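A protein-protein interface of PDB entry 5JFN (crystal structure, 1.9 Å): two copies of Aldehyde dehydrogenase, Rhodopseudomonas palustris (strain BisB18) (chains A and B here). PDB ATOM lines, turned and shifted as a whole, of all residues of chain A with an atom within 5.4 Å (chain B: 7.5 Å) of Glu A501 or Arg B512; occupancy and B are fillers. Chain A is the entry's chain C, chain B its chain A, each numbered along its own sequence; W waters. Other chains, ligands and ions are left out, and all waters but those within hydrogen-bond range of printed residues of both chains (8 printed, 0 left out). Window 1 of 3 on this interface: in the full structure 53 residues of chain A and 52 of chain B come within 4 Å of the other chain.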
ATOM      1  N   LYS A 292     -14.279   6.467   9.780  1.00  0.00           N
ATOM      2  CA  LYS A 292     -15.441   5.800  10.349  1.00  0.00           C
ATOM      3  C   LYS A 292     -16.676   6.659  10.131  1.00  0.00           C
ATOM      4  O   LYS A 292     -16.652   7.875  10.345  1.00  0.00           O
ATOM      5  CB  LYS A 292     -15.281   5.512  11.839  1.00  0.00           C
ATOM      6  CG  LYS A 292     -16.421   4.584  12.308  1.00  0.00           C
ATOM      7  CD  LYS A 292     -16.681   4.635  13.784  1.00  0.00           C
ATOM      8  CE  LYS A 292     -17.930   3.827  14.127  1.00  0.00           C
ATOM      9  NZ  LYS A 292     -17.817   2.385  13.782  1.00  0.00           N
ATOM     10  N   ALA A 293     -17.756   6.026   9.696  1.00  0.00           N
ATOM     11  CA  ALA A 293     -19.000   6.736   9.456  1.00  0.00           C
ATOM     12  C   ALA A 293     -20.168   5.901   9.949  1.00  0.00           C
ATOM     13  O   ALA A 293     -20.198   4.683   9.752  1.00  0.00           O
ATOM     14  CB  ALA A 293     -19.185   7.067   7.969  1.00  0.00           C
ATOM     15  N   ILE A 294     -21.116   6.566  10.603  1.00  0.00           N
ATOM     16  CA  ILE A 294     -22.424   5.998  10.909  1.00  0.00           C
ATOM     17  C   ILE A 294     -23.403   6.500   9.859  1.00  0.00           C
ATOM     18  O   ILE A 294     -23.540   7.713   9.652  1.00  0.00           O
ATOM     19  CB  ILE A 294     -22.890   6.379  12.324  1.00  0.00           C
ATOM     20  CG1 ILE A 294     -21.920   5.812  13.367  1.00  0.00           C
ATOM     21  CG2 ILE A 294     -24.327   5.894  12.561  1.00  0.00           C
ATOM     22  CD1 ILE A 294     -22.288   6.142  14.799  1.00  0.00           C
ATOM     23  N   GLY A 295     -24.082   5.573   9.195  1.00  0.00           N
ATOM     24  CA  GLY A 295     -24.984   5.942   8.126  1.00  0.00           C
ATOM     25  C   GLY A 295     -26.404   5.532   8.437  1.00  0.00           C
ATOM     26  O   GLY A 295     -26.696   4.342   8.592  1.00  0.00           O
ATOM     27  N   THR A 471     -34.022  -2.877  11.617  1.00  0.00           N
ATOM     28  CA  THR A 471     -33.441  -2.204  12.771  1.00  0.00           C
ATOM     29  C   THR A 471     -34.496  -1.883  13.818  1.00  0.00           C
ATOM     30  O   THR A 471     -34.215  -1.924  15.024  1.00  0.00           O
ATOM     31  CB  THR A 471     -32.737  -0.932  12.299  1.00  0.00           C
ATOM     32  OG1 THR A 471     -31.623  -1.297  11.475  1.00  0.00           O
ATOM     33  CG2 THR A 471     -32.262  -0.082  13.479  1.00  0.00           C
ATOM     34  N   ALA A 496     -29.524   3.820  12.496  1.00  0.00           N
ATOM     35  CA  ALA A 496     -28.467   3.297  11.633  1.00  0.00           C
ATOM     36  C   ALA A 496     -28.758   1.839  11.281  1.00  0.00           C
ATOM     37  O   ALA A 496     -28.470   0.921  12.060  1.00  0.00           O
ATOM     38  CB  ALA A 496     -27.105   3.446  12.305  1.00  0.00           C
ATOM     39  N   GLY A 497     -29.313   1.636  10.090  1.00  0.00           N
ATOM     40  CA  GLY A 497     -29.416   0.322   9.495  1.00  0.00           C
ATOM     41  C   GLY A 497     -28.138  -0.164   8.815  1.00  0.00           C
ATOM     42  O   GLY A 497     -27.601  -1.220   9.165  1.00  0.00           O
ATOM     43  N   THR A 499     -24.890   0.730   8.762  1.00  0.00           N
ATOM     44  CA  THR A 499     -23.697   0.534   9.566  1.00  0.00           C
ATOM     45  C   THR A 499     -23.995  -0.199  10.867  1.00  0.00           C
ATOM     46  O   THR A 499     -23.076  -0.444  11.650  1.00  0.00           O
ATOM     47  CB  THR A 499     -23.017   1.882   9.835  1.00  0.00           C
ATOM     48  OG1 THR A 499     -23.982   2.823  10.319  1.00  0.00           O
ATOM     49  CG2 THR A 499     -22.406   2.423   8.544  1.00  0.00           C
ATOM     50  N   GLY A 500     -25.260  -0.542  11.115  1.00  0.00           N
ATOM     51  CA  GLY A 500     -25.619  -1.505  12.136  1.00  0.00           C
ATOM     52  C   GLY A 500     -25.675  -1.010  13.568  1.00  0.00           C
ATOM     53  O   GLY A 500     -25.908  -1.826  14.468  1.00  0.00           O
ATOM     54  N   GLU A 501     -25.482   0.286  13.827  1.00  0.00           N
ATOM     55  CA  GLU A 501     -25.538   0.731  15.219  1.00  0.00           C
ATOM     56  C   GLU A 501     -26.954   0.750  15.774  1.00  0.00           C
ATOM     57  O   GLU A 501     -27.125   0.829  16.996  1.00  0.00           O
ATOM     58  CB  GLU A 501     -24.926   2.126  15.383  1.00  0.00           C
ATOM     59  CG  GLU A 501     -23.439   2.199  15.083  1.00  0.00           C
ATOM     60  CD  GLU A 501     -23.143   2.185  13.599  1.00  0.00           C
ATOM     61  OE1 GLU A 501     -24.100   2.295  12.792  1.00  0.00           O
ATOM     62  OE2 GLU A 501     -21.953   2.053  13.242  1.00  0.00           O
ATOM     63  N   GLY A 502     -27.970   0.660  14.920  1.00  0.00           N
ATOM     64  CA  GLY A 502     -29.331   0.709  15.415  1.00  0.00           C
ATOM     65  C   GLY A 502     -29.707   2.118  15.827  1.00  0.00           C
ATOM     66  O   GLY A 502     -29.436   3.094  15.118  1.00  0.00           O
ATOM     67  N   LEU A 503     -30.340   2.231  16.987  1.00  0.00           N
ATOM     68  CA  LEU A 503     -30.776   3.535  17.472  1.00  0.00           C
ATOM     69  C   LEU A 503     -29.571   4.198  18.121  1.00  0.00           C
ATOM     70  O   LEU A 503     -29.191   3.859  19.242  1.00  0.00           O
ATOM     71  CB  LEU A 503     -31.941   3.396  18.442  1.00  0.00           C
ATOM     72  CG  LEU A 503     -33.316   3.247  17.775  1.00  0.00           C
ATOM     73  CD1 LEU A 503     -33.519   1.825  17.283  1.00  0.00           C
ATOM     74  CD2 LEU A 503     -34.431   3.674  18.738  1.00  0.00           C
ATOM     75  N   THR A 504     -28.958   5.135  17.404  1.00  0.00           N
ATOM     76  CA  THR A 504     -27.731   5.740  17.896  1.00  0.00           C
ATOM     77  C   THR A 504     -27.996   6.489  19.190  1.00  0.00           C
ATOM     78  O   THR A 504     -29.044   7.122  19.365  1.00  0.00           O
ATOM     79  CB  THR A 504     -27.127   6.689  16.864  1.00  0.00           C
ATOM     80  OG1 THR A 504     -28.064   7.726  16.562  1.00  0.00           O
ATOM     81  CG2 THR A 504     -26.744   5.926  15.590  1.00  0.00           C
ATOM     82  N   SER A 508     -22.895   5.070  20.821  1.00  0.00           N
ATOM     83  CA  SER A 508     -22.550   4.940  19.411  1.00  0.00           C
ATOM     84  C   SER A 508     -21.466   5.919  19.001  1.00  0.00           C
ATOM     85  O   SER A 508     -20.786   5.694  17.996  1.00  0.00           O
ATOM     86  CB  SER A 508     -23.780   5.174  18.532  1.00  0.00           C
ATOM     87  OG  SER A 508     -24.930   4.577  19.089  1.00  0.00           O
ATOM     88  N   ASP B 172     -30.798  -7.269  25.284  1.00  0.00           N
ATOM     89  CA  ASP B 172     -31.246  -6.230  26.205  1.00  0.00           C
ATOM     90  C   ASP B 172     -32.768  -6.222  26.214  1.00  0.00           C
ATOM     91  O   ASP B 172     -33.396  -6.397  25.166  1.00  0.00           O
ATOM     92  CB  ASP B 172     -30.749  -4.844  25.789  1.00  0.00           C
ATOM     93  CG  ASP B 172     -29.238  -4.735  25.757  1.00  0.00           C
ATOM     94  OD1 ASP B 172     -28.564  -5.478  26.494  1.00  0.00           O
ATOM     95  OD2 ASP B 172     -28.733  -3.882  24.997  1.00  0.00           O
ATOM     96  N   VAL B 183     -33.699  -5.800  22.392  1.00  0.00           N
ATOM     97  CA  VAL B 183     -32.623  -5.362  21.518  1.00  0.00           C
ATOM     98  C   VAL B 183     -31.711  -6.563  21.298  1.00  0.00           C
ATOM     99  O   VAL B 183     -31.204  -7.146  22.263  1.00  0.00           O
ATOM    100  CB  VAL B 183     -31.861  -4.169  22.116  1.00  0.00           C
ATOM    101  CG1 VAL B 183     -30.782  -3.719  21.175  1.00  0.00           C
ATOM    102  CG2 VAL B 183     -32.829  -3.012  22.427  1.00  0.00           C
ATOM    103  N   GLU B 184     -31.531  -6.951  20.037  1.00  0.00           N
ATOM    104  CA  GLU B 184     -30.797  -8.160  19.683  1.00  0.00           C
ATOM    105  C   GLU B 184     -29.706  -7.842  18.670  1.00  0.00           C
ATOM    106  O   GLU B 184     -29.766  -6.835  17.962  1.00  0.00           O
ATOM    107  CB  GLU B 184     -31.724  -9.228  19.083  1.00  0.00           C
ATOM    108  CG  GLU B 184     -32.899  -9.611  19.957  1.00  0.00           C
ATOM    109  CD  GLU B 184     -32.564 -10.707  20.954  1.00  0.00           C
ATOM    110  OE1 GLU B 184     -31.371 -10.863  21.308  1.00  0.00           O
ATOM    111  OE2 GLU B 184     -33.501 -11.416  21.383  1.00  0.00           O
ATOM    112  N   TYR B 185     -28.723  -8.742  18.590  1.00  0.00           N
ATOM    113  CA  TYR B 185     -27.626  -8.665  17.629  1.00  0.00           C
ATOM    114  C   TYR B 185     -27.865  -9.662  16.504  1.00  0.00           C
ATOM    115  O   TYR B 185     -27.843 -10.874  16.737  1.00  0.00           O
ATOM    116  CB  TYR B 185     -26.288  -8.967  18.298  1.00  0.00           C
ATOM    117  CG  TYR B 185     -25.793  -7.895  19.228  1.00  0.00           C
ATOM    118  CD1 TYR B 185     -25.265  -6.710  18.733  1.00  0.00           C
ATOM    119  CD2 TYR B 185     -25.844  -8.070  20.608  1.00  0.00           C
ATOM    120  CE1 TYR B 185     -24.800  -5.725  19.589  1.00  0.00           C
ATOM    121  CE2 TYR B 185     -25.382  -7.092  21.470  1.00  0.00           C
ATOM    122  CZ  TYR B 185     -24.861  -5.920  20.955  1.00  0.00           C
ATOM    123  OH  TYR B 185     -24.400  -4.944  21.810  1.00  0.00           O
ATOM    124  N   SER B 186     -28.047  -9.157  15.289  1.00  0.00           N
ATOM    125  CA  SER B 186     -28.425  -9.956  14.133  1.00  0.00           C
ATOM    126  C   SER B 186     -27.371  -9.854  13.029  1.00  0.00           C
ATOM    127  O   SER B 186     -26.539  -8.942  13.046  1.00  0.00           O
ATOM    128  CB  SER B 186     -29.793  -9.495  13.609  1.00  0.00           C
ATOM    129  OG  SER B 186     -30.817  -9.831  14.532  1.00  0.00           O
ATOM    130  N   PRO B 187     -27.386 -10.767  12.050  1.00  0.00           N
ATOM    131  CA  PRO B 187     -26.317 -10.792  11.039  1.00  0.00           C
ATOM    132  C   PRO B 187     -26.298  -9.560  10.154  1.00  0.00           C
ATOM    133  O   PRO B 187     -27.328  -8.940   9.883  1.00  0.00           O
ATOM    134  CB  PRO B 187     -26.642 -12.036  10.195  1.00  0.00           C
ATOM    135  CG  PRO B 187     -27.625 -12.818  10.968  1.00  0.00           C
ATOM    136  CD  PRO B 187     -28.309 -11.911  11.922  1.00  0.00           C
ATOM    137  N   PHE B 188     -25.092  -9.217   9.687  1.00  0.00           N
ATOM    138  CA  PHE B 188     -24.977  -8.304   8.554  1.00  0.00           C
ATOM    139  C   PHE B 188     -25.294  -9.021   7.250  1.00  0.00           C
ATOM    140  O   PHE B 188     -26.057  -8.519   6.418  1.00  0.00           O
ATOM    141  CB  PHE B 188     -23.572  -7.701   8.491  1.00  0.00           C
ATOM    142  CG  PHE B 188     -23.406  -6.462   9.318  1.00  0.00           C
ATOM    143  CD1 PHE B 188     -23.737  -5.221   8.801  1.00  0.00           C
ATOM    144  CD2 PHE B 188     -22.901  -6.536  10.606  1.00  0.00           C
ATOM    145  CE1 PHE B 188     -23.579  -4.075   9.556  1.00  0.00           C
ATOM    146  CE2 PHE B 188     -22.742  -5.392  11.368  1.00  0.00           C
ATOM    147  CZ  PHE B 188     -23.085  -4.159  10.837  1.00  0.00           C
ATOM    148  N   LYS B 292     -20.037  -0.334   5.137  1.00  0.00           N
ATOM    149  CA  LYS B 292     -19.664  -0.510   6.536  1.00  0.00           C
ATOM    150  C   LYS B 292     -18.332  -1.239   6.620  1.00  0.00           C
ATOM    151  O   LYS B 292     -18.157  -2.300   6.017  1.00  0.00           O
ATOM    152  CB  LYS B 292     -20.744  -1.307   7.269  1.00  0.00           C
ATOM    153  CG  LYS B 292     -20.333  -1.820   8.651  1.00  0.00           C
ATOM    154  CD  LYS B 292     -20.209  -0.688   9.657  1.00  0.00           C
ATOM    155  CE  LYS B 292     -20.100  -1.208  11.086  1.00  0.00           C
ATOM    156  NZ  LYS B 292     -20.216  -0.097  12.091  1.00  0.00           N
ATOM    157  N   THR B 499     -12.143   2.842  13.751  1.00  0.00           N
ATOM    158  CA  THR B 499     -13.583   2.615  13.775  1.00  0.00           C
ATOM    159  C   THR B 499     -14.138   2.353  15.173  1.00  0.00           C
ATOM    160  O   THR B 499     -15.357   2.254  15.326  1.00  0.00           O
ATOM    161  CB  THR B 499     -13.961   1.473  12.815  1.00  0.00           C
ATOM    162  OG1 THR B 499     -13.180   0.308  13.101  1.00  0.00           O
ATOM    163  CG2 THR B 499     -13.711   1.899  11.371  1.00  0.00           C
ATOM    164  N   GLU B 501     -14.429   0.052  17.560  1.00  0.00           N
ATOM    165  CA  GLU B 501     -15.071  -1.109  18.173  1.00  0.00           C
ATOM    166  C   GLU B 501     -14.226  -1.743  19.272  1.00  0.00           C
ATOM    167  O   GLU B 501     -14.751  -2.564  20.027  1.00  0.00           O
ATOM    168  CB  GLU B 501     -15.392  -2.174  17.118  1.00  0.00           C
ATOM    169  CG  GLU B 501     -16.447  -1.765  16.102  1.00  0.00           C
ATOM    170  CD  GLU B 501     -15.870  -0.946  14.959  1.00  0.00           C
ATOM    171  OE1 GLU B 501     -14.632  -0.807  14.898  1.00  0.00           O
ATOM    172  OE2 GLU B 501     -16.654  -0.447  14.121  1.00  0.00           O
ATOM    173  N   LYS B 507     -20.377  -9.620  18.524  1.00  0.00           N
ATOM    174  CA  LYS B 507     -21.216  -8.421  18.566  1.00  0.00           C
ATOM    175  C   LYS B 507     -20.818  -7.416  17.494  1.00  0.00           C
ATOM    176  O   LYS B 507     -21.678  -6.770  16.880  1.00  0.00           O
ATOM    177  CB  LYS B 507     -21.096  -7.719  19.925  1.00  0.00           C
ATOM    178  CG  LYS B 507     -21.795  -8.308  21.124  1.00  0.00           C
ATOM    179  CD  LYS B 507     -21.576  -7.336  22.304  1.00  0.00           C
ATOM    180  CE  LYS B 507     -22.281  -7.759  23.595  1.00  0.00           C
ATOM    181  NZ  LYS B 507     -21.583  -8.872  24.312  1.00  0.00           N
ATOM    182  N   SER B 508     -19.507  -7.223  17.307  1.00  0.00           N
ATOM    183  CA  SER B 508     -19.006  -6.255  16.342  1.00  0.00           C
ATOM    184  C   SER B 508     -19.433  -6.597  14.925  1.00  0.00           C
ATOM    185  O   SER B 508     -19.452  -5.716  14.058  1.00  0.00           O
ATOM    186  CB  SER B 508     -17.474  -6.185  16.393  1.00  0.00           C
ATOM    187  OG  SER B 508     -16.986  -6.226  17.726  1.00  0.00           O
ATOM    188  N   ALA B 510     -22.386  -7.751  14.060  1.00  0.00           N
ATOM    189  CA  ALA B 510     -23.825  -7.904  14.117  1.00  0.00           C
ATOM    190  C   ALA B 510     -24.483  -6.536  14.058  1.00  0.00           C
ATOM    191  O   ALA B 510     -23.897  -5.526  14.463  1.00  0.00           O
ATOM    192  CB  ALA B 510     -24.262  -8.647  15.381  1.00  0.00           C
ATOM    193  N   ARG B 511     -25.700  -6.520  13.517  1.00  0.00           N
ATOM    194  CA  ARG B 511     -26.529  -5.327  13.468  1.00  0.00           C
ATOM    195  C   ARG B 511     -27.433  -5.325  14.688  1.00  0.00           C
ATOM    196  O   ARG B 511     -28.044  -6.345  15.016  1.00  0.00           O
ATOM    197  CB  ARG B 511     -27.389  -5.288  12.203  1.00  0.00           C
ATOM    198  CG  ARG B 511     -26.633  -5.266  10.893  1.00  0.00           C
ATOM    199  CD  ARG B 511     -27.589  -5.456   9.712  1.00  0.00           C
ATOM    200  NE  ARG B 511     -28.502  -4.332   9.541  1.00  0.00           N
ATOM    201  CZ  ARG B 511     -29.818  -4.383   9.732  1.00  0.00           C
ATOM    202  NH1 ARG B 511     -30.405  -5.510  10.108  1.00  0.00           N
ATOM    203  NH2 ARG B 511     -30.551  -3.295   9.541  1.00  0.00           N
ATOM    204  N   ARG B 512     -27.522  -4.176  15.348  1.00  0.00           N
ATOM    205  CA  ARG B 512     -28.356  -4.034  16.531  1.00  0.00           C
ATOM    206  C   ARG B 512     -29.792  -3.772  16.091  1.00  0.00           C
ATOM    207  O   ARG B 512     -30.050  -2.834  15.330  1.00  0.00           O
ATOM    208  CB  ARG B 512     -27.826  -2.903  17.410  1.00  0.00           C
ATOM    209  CG  ARG B 512     -28.505  -2.800  18.761  1.00  0.00           C
ATOM    210  CD  ARG B 512     -27.801  -1.806  19.682  1.00  0.00           C
ATOM    211  NE  ARG B 512     -26.472  -2.261  20.084  1.00  0.00           N
ATOM    212  CZ  ARG B 512     -25.331  -1.760  19.616  1.00  0.00           C
ATOM    213  NH1 ARG B 512     -24.171  -2.236  20.047  1.00  0.00           N
ATOM    214  NH2 ARG B 512     -25.348  -0.780  18.719  1.00  0.00           N
ATOM    215  N   ARG B 513     -30.720  -4.609  16.549  1.00  0.00           N
ATOM    216  CA  ARG B 513     -32.116  -4.534  16.142  1.00  0.00           C
ATOM    217  C   ARG B 513     -33.000  -4.382  17.365  1.00  0.00           C
ATOM    218  O   ARG B 513     -32.717  -4.954  18.420  1.00  0.00           O
ATOM    219  CB  ARG B 513     -32.524  -5.779  15.350  1.00  0.00           C
ATOM    220  CG  ARG B 513     -31.822  -5.903  14.019  1.00  0.00           C
ATOM    221  CD  ARG B 513     -32.335  -7.096  13.235  1.00  0.00           C
ATOM    222  NE  ARG B 513     -33.784  -7.228  13.323  1.00  0.00           N
ATOM    223  CZ  ARG B 513     -34.394  -8.268  13.880  1.00  0.00           C
ATOM    224  NH1 ARG B 513     -33.669  -9.262  14.385  1.00  0.00           N
ATOM    225  NH2 ARG B 513     -35.719  -8.319  13.930  1.00  0.00           N
ATOM    226  N   LYS B 514     -34.072  -3.611  17.213  1.00  0.00           N
ATOM    227  CA  LYS B 514     -34.959  -3.261  18.311  1.00  0.00           C
ATOM    228  C   LYS B 514     -36.359  -3.747  17.976  1.00  0.00           C
ATOM    229  O   LYS B 514     -36.902  -3.398  16.925  1.00  0.00           O
ATOM    230  CB  LYS B 514     -34.952  -1.746  18.545  1.00  0.00           C
ATOM    231  CG  LYS B 514     -35.874  -1.253  19.646  1.00  0.00           C
ATOM    232  CD  LYS B 514     -35.882   0.281  19.663  1.00  0.00           C
ATOM    233  CE  LYS B 514     -36.751   0.843  20.767  1.00  0.00           C
ATOM    234  NZ  LYS B 514     -36.730   2.338  20.744  1.00  0.00           N
HETATM  235  O   HOH W   1     -31.967  -1.077  16.546  1.00  0.00           O
HETATM  236  O   HOH W   2     -29.326  -2.056  12.668  1.00  0.00           O
HETATM  237  O   HOH W   3     -22.574  -1.335  14.350  1.00  0.00           O
HETATM  238  O   HOH W   4     -17.576   1.706  16.924  1.00  0.00           O
HETATM  239  O   HOH W   5     -19.420   2.392  11.347  1.00  0.00           O
HETATM  240  O   HOH W   6     -20.214   1.745  14.982  1.00  0.00           O
HETATM  241  O   HOH W   7     -24.398   2.074  19.216  1.00  0.00           O
HETATM  242  O   HOH W   8     -17.395   0.687  11.589  1.00  0.00           O
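Lys B292 touches its own counterpart, Lys A292.
Lys A292 touches Thr B499, and with the chains exchanged Thr A499 touches Lys B292.
Lys A292 touches Glu B501, and with the chains exchanged Glu A501 touches Lys B292.
Positions printed for both chains: 292, 499, 501 and 508.
Among the printed residues, merely in contact across the chains: Lys A292 with Lys B292, Thr A471 with Arg B512, Thr A471 with Arg B513, Thr A499 with Phe B188, Gly A500 with Phe B188, Gly A500 with Arg B511, Gly A502 with Arg B512 and Leu A503 with Lys B514.
Of the printed residues of chain B, Lys A292 touches Lys B292 (3.8 Å), Thr B499 (2.9 Å) and Glu B501 (3.1 Å).
Of the printed residues of chain B, Glu A501 touches Lys B292 and Arg B512.
Printed residues of chain A within 4 Å of Lys B292: Lys A292 (3.8 Å), Thr A499 (2.9 Å) and Glu A501 (3.0 Å).
Printed residues of chain A within 4 Å of Thr B499: Lys A292.
Of the printed residues of chain A, Arg B512 touches Thr A471 (3.99 Å), Gly A500 (3.0 Å), Glu A501 (3.0 Å) and Gly A502 (3.6 Å).
Printed residues of chain A within 4 Å of Lys B514: Thr A471 and Leu A503.
The nearest printed residue of chain A that does not touch Thr B499 is Ala A293 (6.0 Å).
Along chain A the printed residues that touch a printed residue of chain B span positions 292 to 503.
Of the 17 printed residues of chain B, 8 touch a printed residue of chain A.
Among the printed residues, 17 pairs touch across the chains.
Among the printed residues, Asp or Glu carboxylates within 4 Å of a Lys or Arg side-chain nitrogen of the other chain: Lys A292 with Glu B501 and Glu A501 with Lys B292.
Water W2 lies within hydrogen-bond range of OG1 of Thr A471, O of Arg B512 and O of Ala A496.
Water W5 lies within hydrogen-bond range of the side-chain amino group of Lys B292, the backbone carbonyl oxygen of Ala A293, the side-chain amino group of Lys A292 and the side-chain carboxylate of Glu A501.
Water W4 lies within hydrogen-bond range of the backbone carbonyl oxygen (O) of Thr B499 (2.8 Å) and the side-chain amino group (NZ) of Lys A292 (3.2 Å).
Water W8 lies within hydrogen-bond range of NZ of Lys A292, OE2 of Glu B501 and NZ of Lys B292.
Water W1 lies within hydrogen-bond range of the backbone carbonyl oxygen of Thr A471 (2.8 Å), the backbone carbonyl oxygen of Arg B512 (2.9 Å) and the backbone NH of Lys B514 (3.4 Å).
Water W3 lies within hydrogen-bond range of the backbone carbonyl oxygen of Thr A499 (2.9 Å), the backbone NH of Glu A501 (3.4 Å), the backbone carbonyl oxygen of Gly A500 (3.4 Å) and the side-chain amino group of Lys B292 (3.5 Å).
N of Arg B513 is in hydrogen-bond range of O of Glu B184 (2.8 Å).
OG1 of Thr B499 lies within hydrogen-bond range of OE1 of Glu B501 (2.6 Å).
NH1 of Arg B512 sits at hydrogen-bond distance from OH of Tyr B185, at 3.2 Å.
The guanidinium group (NH1) of Arg B513 lies within hydrogen-bond range of the side-chain hydroxyl (OG) of Ser B186 (2.9 Å).
The backbone carbonyl oxygen (O) of Ser B186 is in hydrogen-bond range of the backbone NH (N) of Arg B511.
O of Gly A502 lies within hydrogen-bond range of N of Ala A496 (2.7 Å).
The side-chain carboxylate (OE2) of Glu A501 lies within salt-bridge range of the side-chain amino group (NZ) of Lys B292, 3.0 Å away.
N of Arg B512 lies within hydrogen-bond range of O of Gly A500 (3.0 Å).
The guanidinium group (NE) of Arg B511 lies within hydrogen-bond range of the backbone carbonyl oxygen (O) of Gly A497, at 3.3 Å.
The guanidinium group of Arg B512 sits at hydrogen-bond distance from the backbone carbonyl oxygen of Glu A501 (3.0 Å).
The backbone carbonyl oxygen (O) of Thr B499 sits at hydrogen-bond distance from the side-chain amino group (NZ) of Lys A292 (2.9 Å).
The side-chain amino group (NZ) of Lys A292 is in salt-bridge range of the side-chain carboxylate (OE2) of Glu B501 (3.1 Å).
N of Lys B514 lies within hydrogen-bond range of O of Thr A471 (2.8 Å).
The side-chain amino group of Lys B292 sits at hydrogen-bond distance from the backbone carbonyl oxygen of Thr A499 (2.9 Å).
The guanidinium group of Arg B511 is in hydrogen-bond range of the side-chain hydroxyl of Thr A471.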
